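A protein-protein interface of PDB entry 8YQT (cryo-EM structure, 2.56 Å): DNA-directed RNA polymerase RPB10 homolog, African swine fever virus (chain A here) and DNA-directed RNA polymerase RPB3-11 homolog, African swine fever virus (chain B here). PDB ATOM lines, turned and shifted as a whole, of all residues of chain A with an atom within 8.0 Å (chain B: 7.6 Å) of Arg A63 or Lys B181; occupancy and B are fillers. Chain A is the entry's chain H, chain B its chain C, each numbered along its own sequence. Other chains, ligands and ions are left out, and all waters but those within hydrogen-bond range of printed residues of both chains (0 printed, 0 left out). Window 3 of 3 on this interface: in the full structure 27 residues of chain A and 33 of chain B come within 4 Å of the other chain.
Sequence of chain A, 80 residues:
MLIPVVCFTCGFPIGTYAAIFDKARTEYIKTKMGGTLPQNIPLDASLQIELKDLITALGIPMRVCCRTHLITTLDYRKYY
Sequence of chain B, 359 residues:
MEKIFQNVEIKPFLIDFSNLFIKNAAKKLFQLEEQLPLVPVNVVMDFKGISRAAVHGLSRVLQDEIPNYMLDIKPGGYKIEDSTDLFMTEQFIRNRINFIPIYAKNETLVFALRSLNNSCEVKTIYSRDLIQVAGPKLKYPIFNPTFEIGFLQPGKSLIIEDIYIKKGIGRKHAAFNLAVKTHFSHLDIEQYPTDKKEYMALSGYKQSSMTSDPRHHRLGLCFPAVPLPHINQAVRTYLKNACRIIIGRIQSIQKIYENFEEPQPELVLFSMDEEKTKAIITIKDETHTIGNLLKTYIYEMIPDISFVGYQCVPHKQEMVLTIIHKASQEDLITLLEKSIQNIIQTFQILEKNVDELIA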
ATOM      1  N   CYS A   7      -1.160  27.752 -36.293  1.00  0.00           N
ATOM      2  CA  CYS A   7      -2.156  26.828 -36.810  1.00  0.00           C
ATOM      3  C   CYS A   7      -3.044  27.529 -37.829  1.00  0.00           C
ATOM      4  O   CYS A   7      -3.516  28.645 -37.601  1.00  0.00           O
ATOM      5  CB  CYS A   7      -2.990  26.272 -35.658  1.00  0.00           C
ATOM      6  SG  CYS A   7      -4.400  25.281 -36.146  1.00  0.00           S
ATOM      7  N   THR A   9      -6.005  26.941 -38.631  1.00  0.00           N
ATOM      8  CA  THR A   9      -7.412  27.010 -38.265  1.00  0.00           C
ATOM      9  C   THR A   9      -7.674  27.985 -37.122  1.00  0.00           C
ATOM     10  O   THR A   9      -8.577  28.820 -37.215  1.00  0.00           O
ATOM     11  CB  THR A   9      -7.920  25.614 -37.901  1.00  0.00           C
ATOM     12  OG1 THR A   9      -7.793  24.750 -39.034  1.00  0.00           O
ATOM     13  CG2 THR A   9      -9.366  25.673 -37.502  1.00  0.00           C
ATOM     14  N   CYS A  10      -6.898  27.902 -36.042  1.00  0.00           N
ATOM     15  CA  CYS A  10      -7.158  28.705 -34.859  1.00  0.00           C
ATOM     16  C   CYS A  10      -6.089  29.744 -34.561  1.00  0.00           C
ATOM     17  O   CYS A  10      -6.359  30.673 -33.796  1.00  0.00           O
ATOM     18  CB  CYS A  10      -7.323  27.805 -33.629  1.00  0.00           C
ATOM     19  SG  CYS A  10      -5.791  27.135 -33.002  1.00  0.00           S
ATOM     20  N   GLY A  11      -4.899  29.618 -35.133  1.00  0.00           N
ATOM     21  CA  GLY A  11      -3.861  30.603 -34.923  1.00  0.00           C
ATOM     22  C   GLY A  11      -2.993  30.399 -33.704  1.00  0.00           C
ATOM     23  O   GLY A  11      -2.275  31.325 -33.319  1.00  0.00           O
ATOM     24  N   PHE A  12      -3.043  29.230 -33.077  1.00  0.00           N
ATOM     25  CA  PHE A  12      -2.139  28.944 -31.975  1.00  0.00           C
ATOM     26  C   PHE A  12      -0.703  28.868 -32.490  1.00  0.00           C
ATOM     27  O   PHE A  12      -0.460  28.313 -33.565  1.00  0.00           O
ATOM     28  CB  PHE A  12      -2.529  27.634 -31.289  1.00  0.00           C
ATOM     29  CG  PHE A  12      -1.679  27.295 -30.099  1.00  0.00           C
ATOM     30  CD1 PHE A  12      -1.954  27.840 -28.857  1.00  0.00           C
ATOM     31  CD2 PHE A  12      -0.603  26.433 -30.222  1.00  0.00           C
ATOM     32  CE1 PHE A  12      -1.172  27.533 -27.767  1.00  0.00           C
ATOM     33  CE2 PHE A  12       0.181  26.128 -29.135  1.00  0.00           C
ATOM     34  CZ  PHE A  12      -0.105  26.677 -27.905  1.00  0.00           C
ATOM     35  N   ILE A  14       1.883  27.298 -33.368  1.00  0.00           N
ATOM     36  CA  ILE A  14       2.402  25.951 -33.584  1.00  0.00           C
ATOM     37  C   ILE A  14       3.883  25.978 -33.939  1.00  0.00           C
ATOM     38  O   ILE A  14       4.642  25.087 -33.541  1.00  0.00           O
ATOM     39  CB  ILE A  14       1.550  25.252 -34.665  1.00  0.00           C
ATOM     40  CG1 ILE A  14       0.344  24.570 -34.024  1.00  0.00           C
ATOM     41  CG2 ILE A  14       2.359  24.278 -35.485  1.00  0.00           C
ATOM     42  CD1 ILE A  14       0.715  23.592 -32.957  1.00  0.00           C
ATOM     43  N   ILE A  55       3.931  15.504 -28.627  1.00  0.00           N
ATOM     44  CA  ILE A  55       3.317  16.814 -28.801  1.00  0.00           C
ATOM     45  C   ILE A  55       2.802  17.345 -27.471  1.00  0.00           C
ATOM     46  O   ILE A  55       2.853  18.555 -27.219  1.00  0.00           O
ATOM     47  CB  ILE A  55       2.199  16.740 -29.855  1.00  0.00           C
ATOM     48  CG1 ILE A  55       2.716  16.087 -31.132  1.00  0.00           C
ATOM     49  CG2 ILE A  55       1.677  18.121 -30.172  1.00  0.00           C
ATOM     50  CD1 ILE A  55       1.623  15.589 -32.041  1.00  0.00           C
ATOM     51  N   ILE A  60       1.941  21.732 -26.467  1.00  0.00           N
ATOM     52  CA  ILE A  60       0.839  22.035 -27.385  1.00  0.00           C
ATOM     53  C   ILE A  60      -0.447  21.416 -26.845  1.00  0.00           C
ATOM     54  O   ILE A  60      -0.429  20.261 -26.388  1.00  0.00           O
ATOM     55  CB  ILE A  60       1.166  21.514 -28.788  1.00  0.00           C
ATOM     56  CG1 ILE A  60       2.284  22.354 -29.403  1.00  0.00           C
ATOM     57  CG2 ILE A  60      -0.058  21.509 -29.685  1.00  0.00           C
ATOM     58  CD1 ILE A  60       2.890  21.755 -30.636  1.00  0.00           C
ATOM     59  N   PRO A  61      -1.577  22.135 -26.863  1.00  0.00           N
ATOM     60  CA  PRO A  61      -2.817  21.587 -26.293  1.00  0.00           C
ATOM     61  C   PRO A  61      -3.351  20.395 -27.069  1.00  0.00           C
ATOM     62  O   PRO A  61      -2.730  19.939 -28.032  1.00  0.00           O
ATOM     63  CB  PRO A  61      -3.790  22.771 -26.360  1.00  0.00           C
ATOM     64  CG  PRO A  61      -2.949  23.967 -26.602  1.00  0.00           C
ATOM     65  CD  PRO A  61      -1.767  23.503 -27.365  1.00  0.00           C
ATOM     66  N   MET A  62      -4.519  19.896 -26.675  1.00  0.00           N
ATOM     67  CA  MET A  62      -5.089  18.702 -27.292  1.00  0.00           C
ATOM     68  C   MET A  62      -6.048  19.061 -28.416  1.00  0.00           C
ATOM     69  O   MET A  62      -7.029  18.359 -28.662  1.00  0.00           O
ATOM     70  CB  MET A  62      -5.782  17.855 -26.230  1.00  0.00           C
ATOM     71  CG  MET A  62      -4.887  16.807 -25.554  1.00  0.00           C
ATOM     72  SD  MET A  62      -4.203  15.402 -26.472  1.00  0.00           S
ATOM     73  CE  MET A  62      -5.230  15.308 -27.923  1.00  0.00           C
ATOM     74  N   ARG A  63      -5.786  20.171 -29.101  1.00  0.00           N
ATOM     75  CA  ARG A  63      -6.662  20.663 -30.154  1.00  0.00           C
ATOM     76  C   ARG A  63      -6.484  19.837 -31.421  1.00  0.00           C
ATOM     77  O   ARG A  63      -5.362  19.490 -31.790  1.00  0.00           O
ATOM     78  CB  ARG A  63      -6.362  22.134 -30.435  1.00  0.00           C
ATOM     79  CG  ARG A  63      -6.233  22.977 -29.181  1.00  0.00           C
ATOM     80  CD  ARG A  63      -5.808  24.400 -29.497  1.00  0.00           C
ATOM     81  NE  ARG A  63      -6.775  25.099 -30.332  1.00  0.00           N
ATOM     82  CZ  ARG A  63      -7.876  25.681 -29.881  1.00  0.00           C
ATOM     83  NH1 ARG A  63      -8.187  25.666 -28.595  1.00  0.00           N
ATOM     84  NH2 ARG A  63      -8.684  26.294 -30.738  1.00  0.00           N
ATOM     85  N   VAL A  64      -7.598  19.524 -32.083  1.00  0.00           N
ATOM     86  CA  VAL A  64      -7.543  18.716 -33.299  1.00  0.00           C
ATOM     87  C   VAL A  64      -6.767  19.440 -34.390  1.00  0.00           C
ATOM     88  O   VAL A  64      -5.884  18.862 -35.034  1.00  0.00           O
ATOM     89  CB  VAL A  64      -8.967  18.358 -33.761  1.00  0.00           C
ATOM     90  CG1 VAL A  64      -8.943  17.755 -35.149  1.00  0.00           C
ATOM     91  CG2 VAL A  64      -9.616  17.402 -32.782  1.00  0.00           C
ATOM     92  N   CYS A  65      -7.076  20.719 -34.602  1.00  0.00           N
ATOM     93  CA  CYS A  65      -6.483  21.469 -35.702  1.00  0.00           C
ATOM     94  C   CYS A  65      -4.974  21.608 -35.545  1.00  0.00           C
ATOM     95  O   CYS A  65      -4.221  21.410 -36.507  1.00  0.00           O
ATOM     96  CB  CYS A  65      -7.137  22.847 -35.782  1.00  0.00           C
ATOM     97  SG  CYS A  65      -7.169  23.748 -34.205  1.00  0.00           S
ATOM     98  N   CYS A  66      -4.517  21.956 -34.342  1.00  0.00           N
ATOM     99  CA  CYS A  66      -3.105  22.252 -34.136  1.00  0.00           C
ATOM    100  C   CYS A  66      -2.250  21.016 -34.361  1.00  0.00           C
ATOM    101  O   CYS A  66      -1.246  21.063 -35.078  1.00  0.00           O
ATOM    102  CB  CYS A  66      -2.891  22.802 -32.729  1.00  0.00           C
ATOM    103  SG  CYS A  66      -3.728  24.351 -32.434  1.00  0.00           S
ATOM    104  N   ARG A  67      -2.640  19.899 -33.751  1.00  0.00           N
ATOM    105  CA  ARG A  67      -1.896  18.665 -33.930  1.00  0.00           C
ATOM    106  C   ARG A  67      -2.016  18.138 -35.352  1.00  0.00           C
ATOM    107  O   ARG A  67      -1.052  17.578 -35.878  1.00  0.00           O
ATOM    108  CB  ARG A  67      -2.366  17.634 -32.913  1.00  0.00           C
ATOM    109  CG  ARG A  67      -1.943  17.993 -31.510  1.00  0.00           C
ATOM    110  CD  ARG A  67      -2.680  17.194 -30.472  1.00  0.00           C
ATOM    111  NE  ARG A  67      -2.312  17.629 -29.132  1.00  0.00           N
ATOM    112  CZ  ARG A  67      -1.537  16.943 -28.308  1.00  0.00           C
ATOM    113  NH1 ARG A  67      -1.044  15.765 -28.644  1.00  0.00           N
ATOM    114  NH2 ARG A  67      -1.250  17.451 -27.115  1.00  0.00           N
ATOM    115  N   THR A  68      -3.169  18.327 -35.996  1.00  0.00           N
ATOM    116  CA  THR A  68      -3.293  17.962 -37.404  1.00  0.00           C
ATOM    117  C   THR A  68      -2.255  18.687 -38.254  1.00  0.00           C
ATOM    118  O   THR A  68      -1.506  18.059 -39.012  1.00  0.00           O
ATOM    119  CB  THR A  68      -4.698  18.284 -37.906  1.00  0.00           C
ATOM    120  OG1 THR A  68      -5.657  17.488 -37.205  1.00  0.00           O
ATOM    121  CG2 THR A  68      -4.801  18.004 -39.379  1.00  0.00           C
ATOM    122  N   HIS A  69      -2.190  20.014 -38.132  1.00  0.00           N
ATOM    123  CA  HIS A  69      -1.279  20.783 -38.972  1.00  0.00           C
ATOM    124  C   HIS A  69       0.176  20.583 -38.580  1.00  0.00           C
ATOM    125  O   HIS A  69       1.056  20.712 -39.434  1.00  0.00           O
ATOM    126  CB  HIS A  69      -1.634  22.269 -38.932  1.00  0.00           C
ATOM    127  CG  HIS A  69      -3.028  22.566 -39.384  1.00  0.00           C
ATOM    128  ND1 HIS A  69      -3.539  22.093 -40.573  1.00  0.00           N
ATOM    129  CD2 HIS A  69      -4.018  23.289 -38.812  1.00  0.00           C
ATOM    130  CE1 HIS A  69      -4.786  22.505 -40.708  1.00  0.00           C
ATOM    131  NE2 HIS A  69      -5.100  23.235 -39.654  1.00  0.00           N
ATOM    132  N   PHE B  13       1.401  27.450 -20.807  1.00  0.00           N
ATOM    133  CA  PHE B  13       1.727  26.228 -21.530  1.00  0.00           C
ATOM    134  C   PHE B  13       3.244  26.106 -21.592  1.00  0.00           C
ATOM    135  O   PHE B  13       3.912  26.950 -22.198  1.00  0.00           O
ATOM    136  CB  PHE B  13       1.130  26.243 -22.936  1.00  0.00           C
ATOM    137  CG  PHE B  13      -0.369  26.153 -22.967  1.00  0.00           C
ATOM    138  CD1 PHE B  13      -1.086  25.846 -21.827  1.00  0.00           C
ATOM    139  CD2 PHE B  13      -1.061  26.394 -24.136  1.00  0.00           C
ATOM    140  CE1 PHE B  13      -2.462  25.771 -21.860  1.00  0.00           C
ATOM    141  CE2 PHE B  13      -2.436  26.321 -24.171  1.00  0.00           C
ATOM    142  CZ  PHE B  13      -3.135  26.007 -23.036  1.00  0.00           C
ATOM    143  N   ASN B  42      -3.308  30.103 -20.856  1.00  0.00           N
ATOM    144  CA  ASN B  42      -4.732  29.811 -20.870  1.00  0.00           C
ATOM    145  C   ASN B  42      -5.393  30.474 -19.668  1.00  0.00           C
ATOM    146  O   ASN B  42      -4.953  30.289 -18.530  1.00  0.00           O
ATOM    147  CB  ASN B  42      -4.973  28.303 -20.841  1.00  0.00           C
ATOM    148  CG  ASN B  42      -6.367  27.931 -21.281  1.00  0.00           C
ATOM    149  OD1 ASN B  42      -7.080  28.744 -21.860  1.00  0.00           O
ATOM    150  ND2 ASN B  42      -6.772  26.704 -20.991  1.00  0.00           N
ATOM    151  N   HIS B  56     -19.986  37.048 -24.538  1.00  0.00           N
ATOM    152  CA  HIS B  56     -19.566  36.674 -25.881  1.00  0.00           C
ATOM    153  C   HIS B  56     -18.996  37.861 -26.646  1.00  0.00           C
ATOM    154  O   HIS B  56     -18.106  37.677 -27.478  1.00  0.00           O
ATOM    155  CB  HIS B  56     -20.726  36.048 -26.649  1.00  0.00           C
ATOM    156  CG  HIS B  56     -20.336  35.516 -27.992  1.00  0.00           C
ATOM    157  ND1 HIS B  56     -19.438  34.483 -28.149  1.00  0.00           N
ATOM    158  CD2 HIS B  56     -20.720  35.873 -29.238  1.00  0.00           C
ATOM    159  CE1 HIS B  56     -19.285  34.229 -29.434  1.00  0.00           C
ATOM    160  NE2 HIS B  56     -20.051  35.057 -30.117  1.00  0.00           N
ATOM    161  N   SER B  59     -15.518  38.050 -25.480  1.00  0.00           N
ATOM    162  CA  SER B  59     -14.749  37.007 -26.152  1.00  0.00           C
ATOM    163  C   SER B  59     -14.412  37.403 -27.585  1.00  0.00           C
ATOM    164  O   SER B  59     -13.271  37.245 -28.028  1.00  0.00           O
ATOM    165  CB  SER B  59     -15.523  35.691 -26.125  1.00  0.00           C
ATOM    166  OG  SER B  59     -14.852  34.694 -26.872  1.00  0.00           O
ATOM    167  N   ARG B  60     -15.391  37.931 -28.322  1.00  0.00           N
ATOM    168  CA  ARG B  60     -15.164  38.324 -29.710  1.00  0.00           C
ATOM    169  C   ARG B  60     -14.133  39.440 -29.813  1.00  0.00           C
ATOM    170  O   ARG B  60     -13.273  39.424 -30.705  1.00  0.00           O
ATOM    171  CB  ARG B  60     -16.480  38.763 -30.351  1.00  0.00           C
ATOM    172  CG  ARG B  60     -17.451  37.638 -30.649  1.00  0.00           C
ATOM    173  CD  ARG B  60     -18.823  38.181 -31.006  1.00  0.00           C
ATOM    174  NE  ARG B  60     -18.779  39.055 -32.171  1.00  0.00           N
ATOM    175  CZ  ARG B  60     -18.982  38.656 -33.418  1.00  0.00           C
ATOM    176  NH1 ARG B  60     -19.274  37.400 -33.702  1.00  0.00           N
ATOM    177  NH2 ARG B  60     -18.884  39.538 -34.404  1.00  0.00           N
ATOM    178  N   GLN B  63     -10.811  38.104 -29.271  1.00  0.00           N
ATOM    179  CA  GLN B  63     -10.368  37.296 -30.403  1.00  0.00           C
ATOM    180  C   GLN B  63      -9.841  38.164 -31.536  1.00  0.00           C
ATOM    181  O   GLN B  63      -8.655  38.107 -31.873  1.00  0.00           O
ATOM    182  CB  GLN B  63     -11.507  36.416 -30.917  1.00  0.00           C
ATOM    183  CG  GLN B  63     -11.955  35.325 -29.979  1.00  0.00           C
ATOM    184  CD  GLN B  63     -13.237  34.680 -30.444  1.00  0.00           C
ATOM    185  OE1 GLN B  63     -13.463  34.524 -31.639  1.00  0.00           O
ATOM    186  NE2 GLN B  63     -14.102  34.335 -29.502  1.00  0.00           N
ATOM    187  N   ASP B  64     -10.713  38.972 -32.153  1.00  0.00           N
ATOM    188  CA  ASP B  64     -10.276  39.666 -33.359  1.00  0.00           C
ATOM    189  C   ASP B  64     -10.803  41.091 -33.483  1.00  0.00           C
ATOM    190  O   ASP B  64     -10.937  41.591 -34.605  1.00  0.00           O
ATOM    191  CB  ASP B  64     -10.667  38.872 -34.608  1.00  0.00           C
ATOM    192  CG  ASP B  64     -12.159  38.734 -34.769  1.00  0.00           C
ATOM    193  OD1 ASP B  64     -12.885  38.907 -33.771  1.00  0.00           O
ATOM    194  OD2 ASP B  64     -12.607  38.446 -35.894  1.00  0.00           O
ATOM    195  N   ALA B 179      -6.634  36.293 -29.161  1.00  0.00           N
ATOM    196  CA  ALA B 179      -6.985  35.147 -28.339  1.00  0.00           C
ATOM    197  C   ALA B 179      -7.607  34.042 -29.179  1.00  0.00           C
ATOM    198  O   ALA B 179      -8.388  34.299 -30.096  1.00  0.00           O
ATOM    199  CB  ALA B 179      -7.947  35.552 -27.222  1.00  0.00           C
ATOM    200  N   VAL B 180      -7.241  32.804 -28.859  1.00  0.00           N
ATOM    201  CA  VAL B 180      -7.880  31.629 -29.434  1.00  0.00           C
ATOM    202  C   VAL B 180      -8.816  31.048 -28.387  1.00  0.00           C
ATOM    203  O   VAL B 180      -8.551  31.103 -27.181  1.00  0.00           O
ATOM    204  CB  VAL B 180      -6.852  30.585 -29.932  1.00  0.00           C
ATOM    205  CG1 VAL B 180      -5.674  31.272 -30.595  1.00  0.00           C
ATOM    206  CG2 VAL B 180      -6.386  29.682 -28.813  1.00  0.00           C
ATOM    207  N   LYS B 181      -9.944  30.519 -28.849  1.00  0.00           N
ATOM    208  CA  LYS B 181     -10.959  29.984 -27.953  1.00  0.00           C
ATOM    209  C   LYS B 181     -10.543  28.612 -27.446  1.00  0.00           C
ATOM    210  O   LYS B 181     -10.185  27.733 -28.233  1.00  0.00           O
ATOM    211  CB  LYS B 181     -12.300  29.884 -28.675  1.00  0.00           C
ATOM    212  CG  LYS B 181     -12.885  31.209 -29.099  1.00  0.00           C
ATOM    213  CD  LYS B 181     -14.142  31.001 -29.917  1.00  0.00           C
ATOM    214  CE  LYS B 181     -13.807  30.575 -31.335  1.00  0.00           C
ATOM    215  NZ  LYS B 181     -13.304  31.692 -32.168  1.00  0.00           N
ATOM    216  N   THR B 182     -10.593  28.424 -26.127  1.00  0.00           N
ATOM    217  CA  THR B 182     -10.338  27.118 -25.541  1.00  0.00           C
ATOM    218  C   THR B 182     -11.524  26.535 -24.793  1.00  0.00           C
ATOM    219  O   THR B 182     -11.562  25.316 -24.602  1.00  0.00           O
ATOM    220  CB  THR B 182      -9.131  27.164 -24.587  1.00  0.00           C
ATOM    221  OG1 THR B 182      -9.456  27.926 -23.422  1.00  0.00           O
ATOM    222  CG2 THR B 182      -7.932  27.783 -25.270  1.00  0.00           C
ATOM    223  N   HIS B 183     -12.487  27.352 -24.370  1.00  0.00           N
ATOM    224  CA  HIS B 183     -13.643  26.822 -23.661  1.00  0.00           C
ATOM    225  C   HIS B 183     -14.758  27.856 -23.624  1.00  0.00           C
ATOM    226  O   HIS B 183     -14.494  29.051 -23.509  1.00  0.00           O
ATOM    227  CB  HIS B 183     -13.282  26.408 -22.231  1.00  0.00           C
ATOM    228  CG  HIS B 183     -14.440  25.871 -21.451  1.00  0.00           C
ATOM    229  ND1 HIS B 183     -14.997  24.637 -21.704  1.00  0.00           N
ATOM    230  CD2 HIS B 183     -15.154  26.405 -20.435  1.00  0.00           C
ATOM    231  CE1 HIS B 183     -16.002  24.432 -20.873  1.00  0.00           C
ATOM    232  NE2 HIS B 183     -16.118  25.489 -20.092  1.00  0.00           N
ATOM    233  N   PHE B 184     -15.999  27.384 -23.700  1.00  0.00           N
ATOM    234  CA  PHE B 184     -17.160  28.227 -23.444  1.00  0.00           C
ATOM    235  C   PHE B 184     -18.304  27.340 -22.986  1.00  0.00           C
ATOM    236  O   PHE B 184     -18.632  26.358 -23.655  1.00  0.00           O
ATOM    237  CB  PHE B 184     -17.568  29.028 -24.683  1.00  0.00           C
ATOM    238  CG  PHE B 184     -18.632  30.049 -24.414  1.00  0.00           C
ATOM    239  CD1 PHE B 184     -18.467  30.988 -23.412  1.00  0.00           C
ATOM    240  CD2 PHE B 184     -19.792  30.076 -25.161  1.00  0.00           C
ATOM    241  CE1 PHE B 184     -19.441  31.927 -23.157  1.00  0.00           C
ATOM    242  CE2 PHE B 184     -20.767  31.015 -24.912  1.00  0.00           C
ATOM    243  CZ  PHE B 184     -20.592  31.942 -23.909  1.00  0.00           C
ATOM    244  N   LEU B 219     -15.680  31.028 -19.528  1.00  0.00           N
ATOM    245  CA  LEU B 219     -15.031  31.359 -20.788  1.00  0.00           C
ATOM    246  C   LEU B 219     -13.529  31.175 -20.651  1.00  0.00           C
ATOM    247  O   LEU B 219     -12.914  31.755 -19.756  1.00  0.00           O
ATOM    248  CB  LEU B 219     -15.349  32.797 -21.201  1.00  0.00           C
ATOM    249  CG  LEU B 219     -14.596  33.346 -22.409  1.00  0.00           C
ATOM    250  CD1 LEU B 219     -14.960  32.573 -23.657  1.00  0.00           C
ATOM    251  CD2 LEU B 219     -14.887  34.821 -22.580  1.00  0.00           C
ATOM    252  N   GLY B 220     -12.937  30.393 -21.543  1.00  0.00           N
ATOM    253  CA  GLY B 220     -11.509  30.172 -21.519  1.00  0.00           C
ATOM    254  C   GLY B 220     -10.862  30.513 -22.840  1.00  0.00           C
ATOM    255  O   GLY B 220     -11.246  29.975 -23.882  1.00  0.00           O
ATOM    256  N   LEU B 221      -9.869  31.396 -22.794  1.00  0.00           N
ATOM    257  CA  LEU B 221      -9.167  31.882 -23.972  1.00  0.00           C
ATOM    258  C   LEU B 221      -7.668  31.732 -23.770  1.00  0.00           C
ATOM    259  O   LEU B 221      -7.163  31.846 -22.652  1.00  0.00           O
ATOM    260  CB  LEU B 221      -9.501  33.353 -24.254  1.00  0.00           C
ATOM    261  CG  LEU B 221     -10.954  33.693 -24.584  1.00  0.00           C
ATOM    262  CD1 LEU B 221     -11.169  35.183 -24.480  1.00  0.00           C
ATOM    263  CD2 LEU B 221     -11.325  33.198 -25.972  1.00  0.00           C
ATOM    264  N   CYS B 222      -6.953  31.484 -24.860  1.00  0.00           N
ATOM    265  CA  CYS B 222      -5.507  31.329 -24.818  1.00  0.00           C
ATOM    266  C   CYS B 222      -4.843  32.502 -25.524  1.00  0.00           C
ATOM    267  O   CYS B 222      -5.178  32.815 -26.670  1.00  0.00           O
ATOM    268  CB  CYS B 222      -5.074  30.010 -25.461  1.00  0.00           C
ATOM    269  SG  CYS B 222      -3.332  29.612 -25.241  1.00  0.00           S
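The backbone carbonyl oxygen (O) of Lys B181 lies within hydrogen-bond range of the guanidinium group (NH1) of Arg A63 (2.9 Å).
The backbone carbonyl oxygen (O) of Val B180 sits at hydrogen-bond distance from the backbone NH (N) of Cys B222, 2.8 Å away. The side-chain sulfur (SG) of Cys A10 lies close to the backbone NH (N) of Phe A12 (3.5 Å). The side-chain sulfur of Cys A10 sits close to the guanidinium group of Arg A63. O of Gly B220 lies within hydrogen-bond range of OG1 of Thr B182, at 2.8 Å. The backbone NH of Cys A7 sits at hydrogen-bond distance from the backbone carbonyl oxygen of Phe A12 (2.9 Å). O of Pro A61 sits at hydrogen-bond distance from NE of Arg A67 (2.6 Å).
Among the printed residues, pairs that only touch across the chains: Cys A10 with Val B180, Phe A12 with Phe B13, Phe A12 with Cys B222, Pro A61 with Phe B13 and Arg A63 with Thr B182.
Of the printed residues of chain B, Phe A12 touches Phe B13 (3.8 Å) and Cys B222 (3.9 Å). Of chain B, only Lys B181 (2.9 Å) and Thr B182 (3.9 Å) come within 4 Å of Arg A63. Cys A66 touches none of the printed residues of chain B. Of the printed residues of chain A, Phe B13 touches Phe A12 and Pro A61. Lys B181 touches just one residue of chain A: Arg A63. The nearest residue of chain B that does not touch Arg A63 is Val B180 (4.4 Å). The nearest residue of chain A that does not touch Lys B181 is Cys A10 (6.1 Å).
Hydrophobic or aromatic side chains of chain B within 4 Å of the printed part of chain A: Phe B13 and Val B180. Along chain B the printed residues that touch a printed residue of chain A span positions 13 to 222. Of the 17 printed residues of chain A, 4 touch a printed residue of chain B. Hydrophobic or aromatic side chains of chain A that line the printed part of chain B: Phe A12 and Pro A61.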
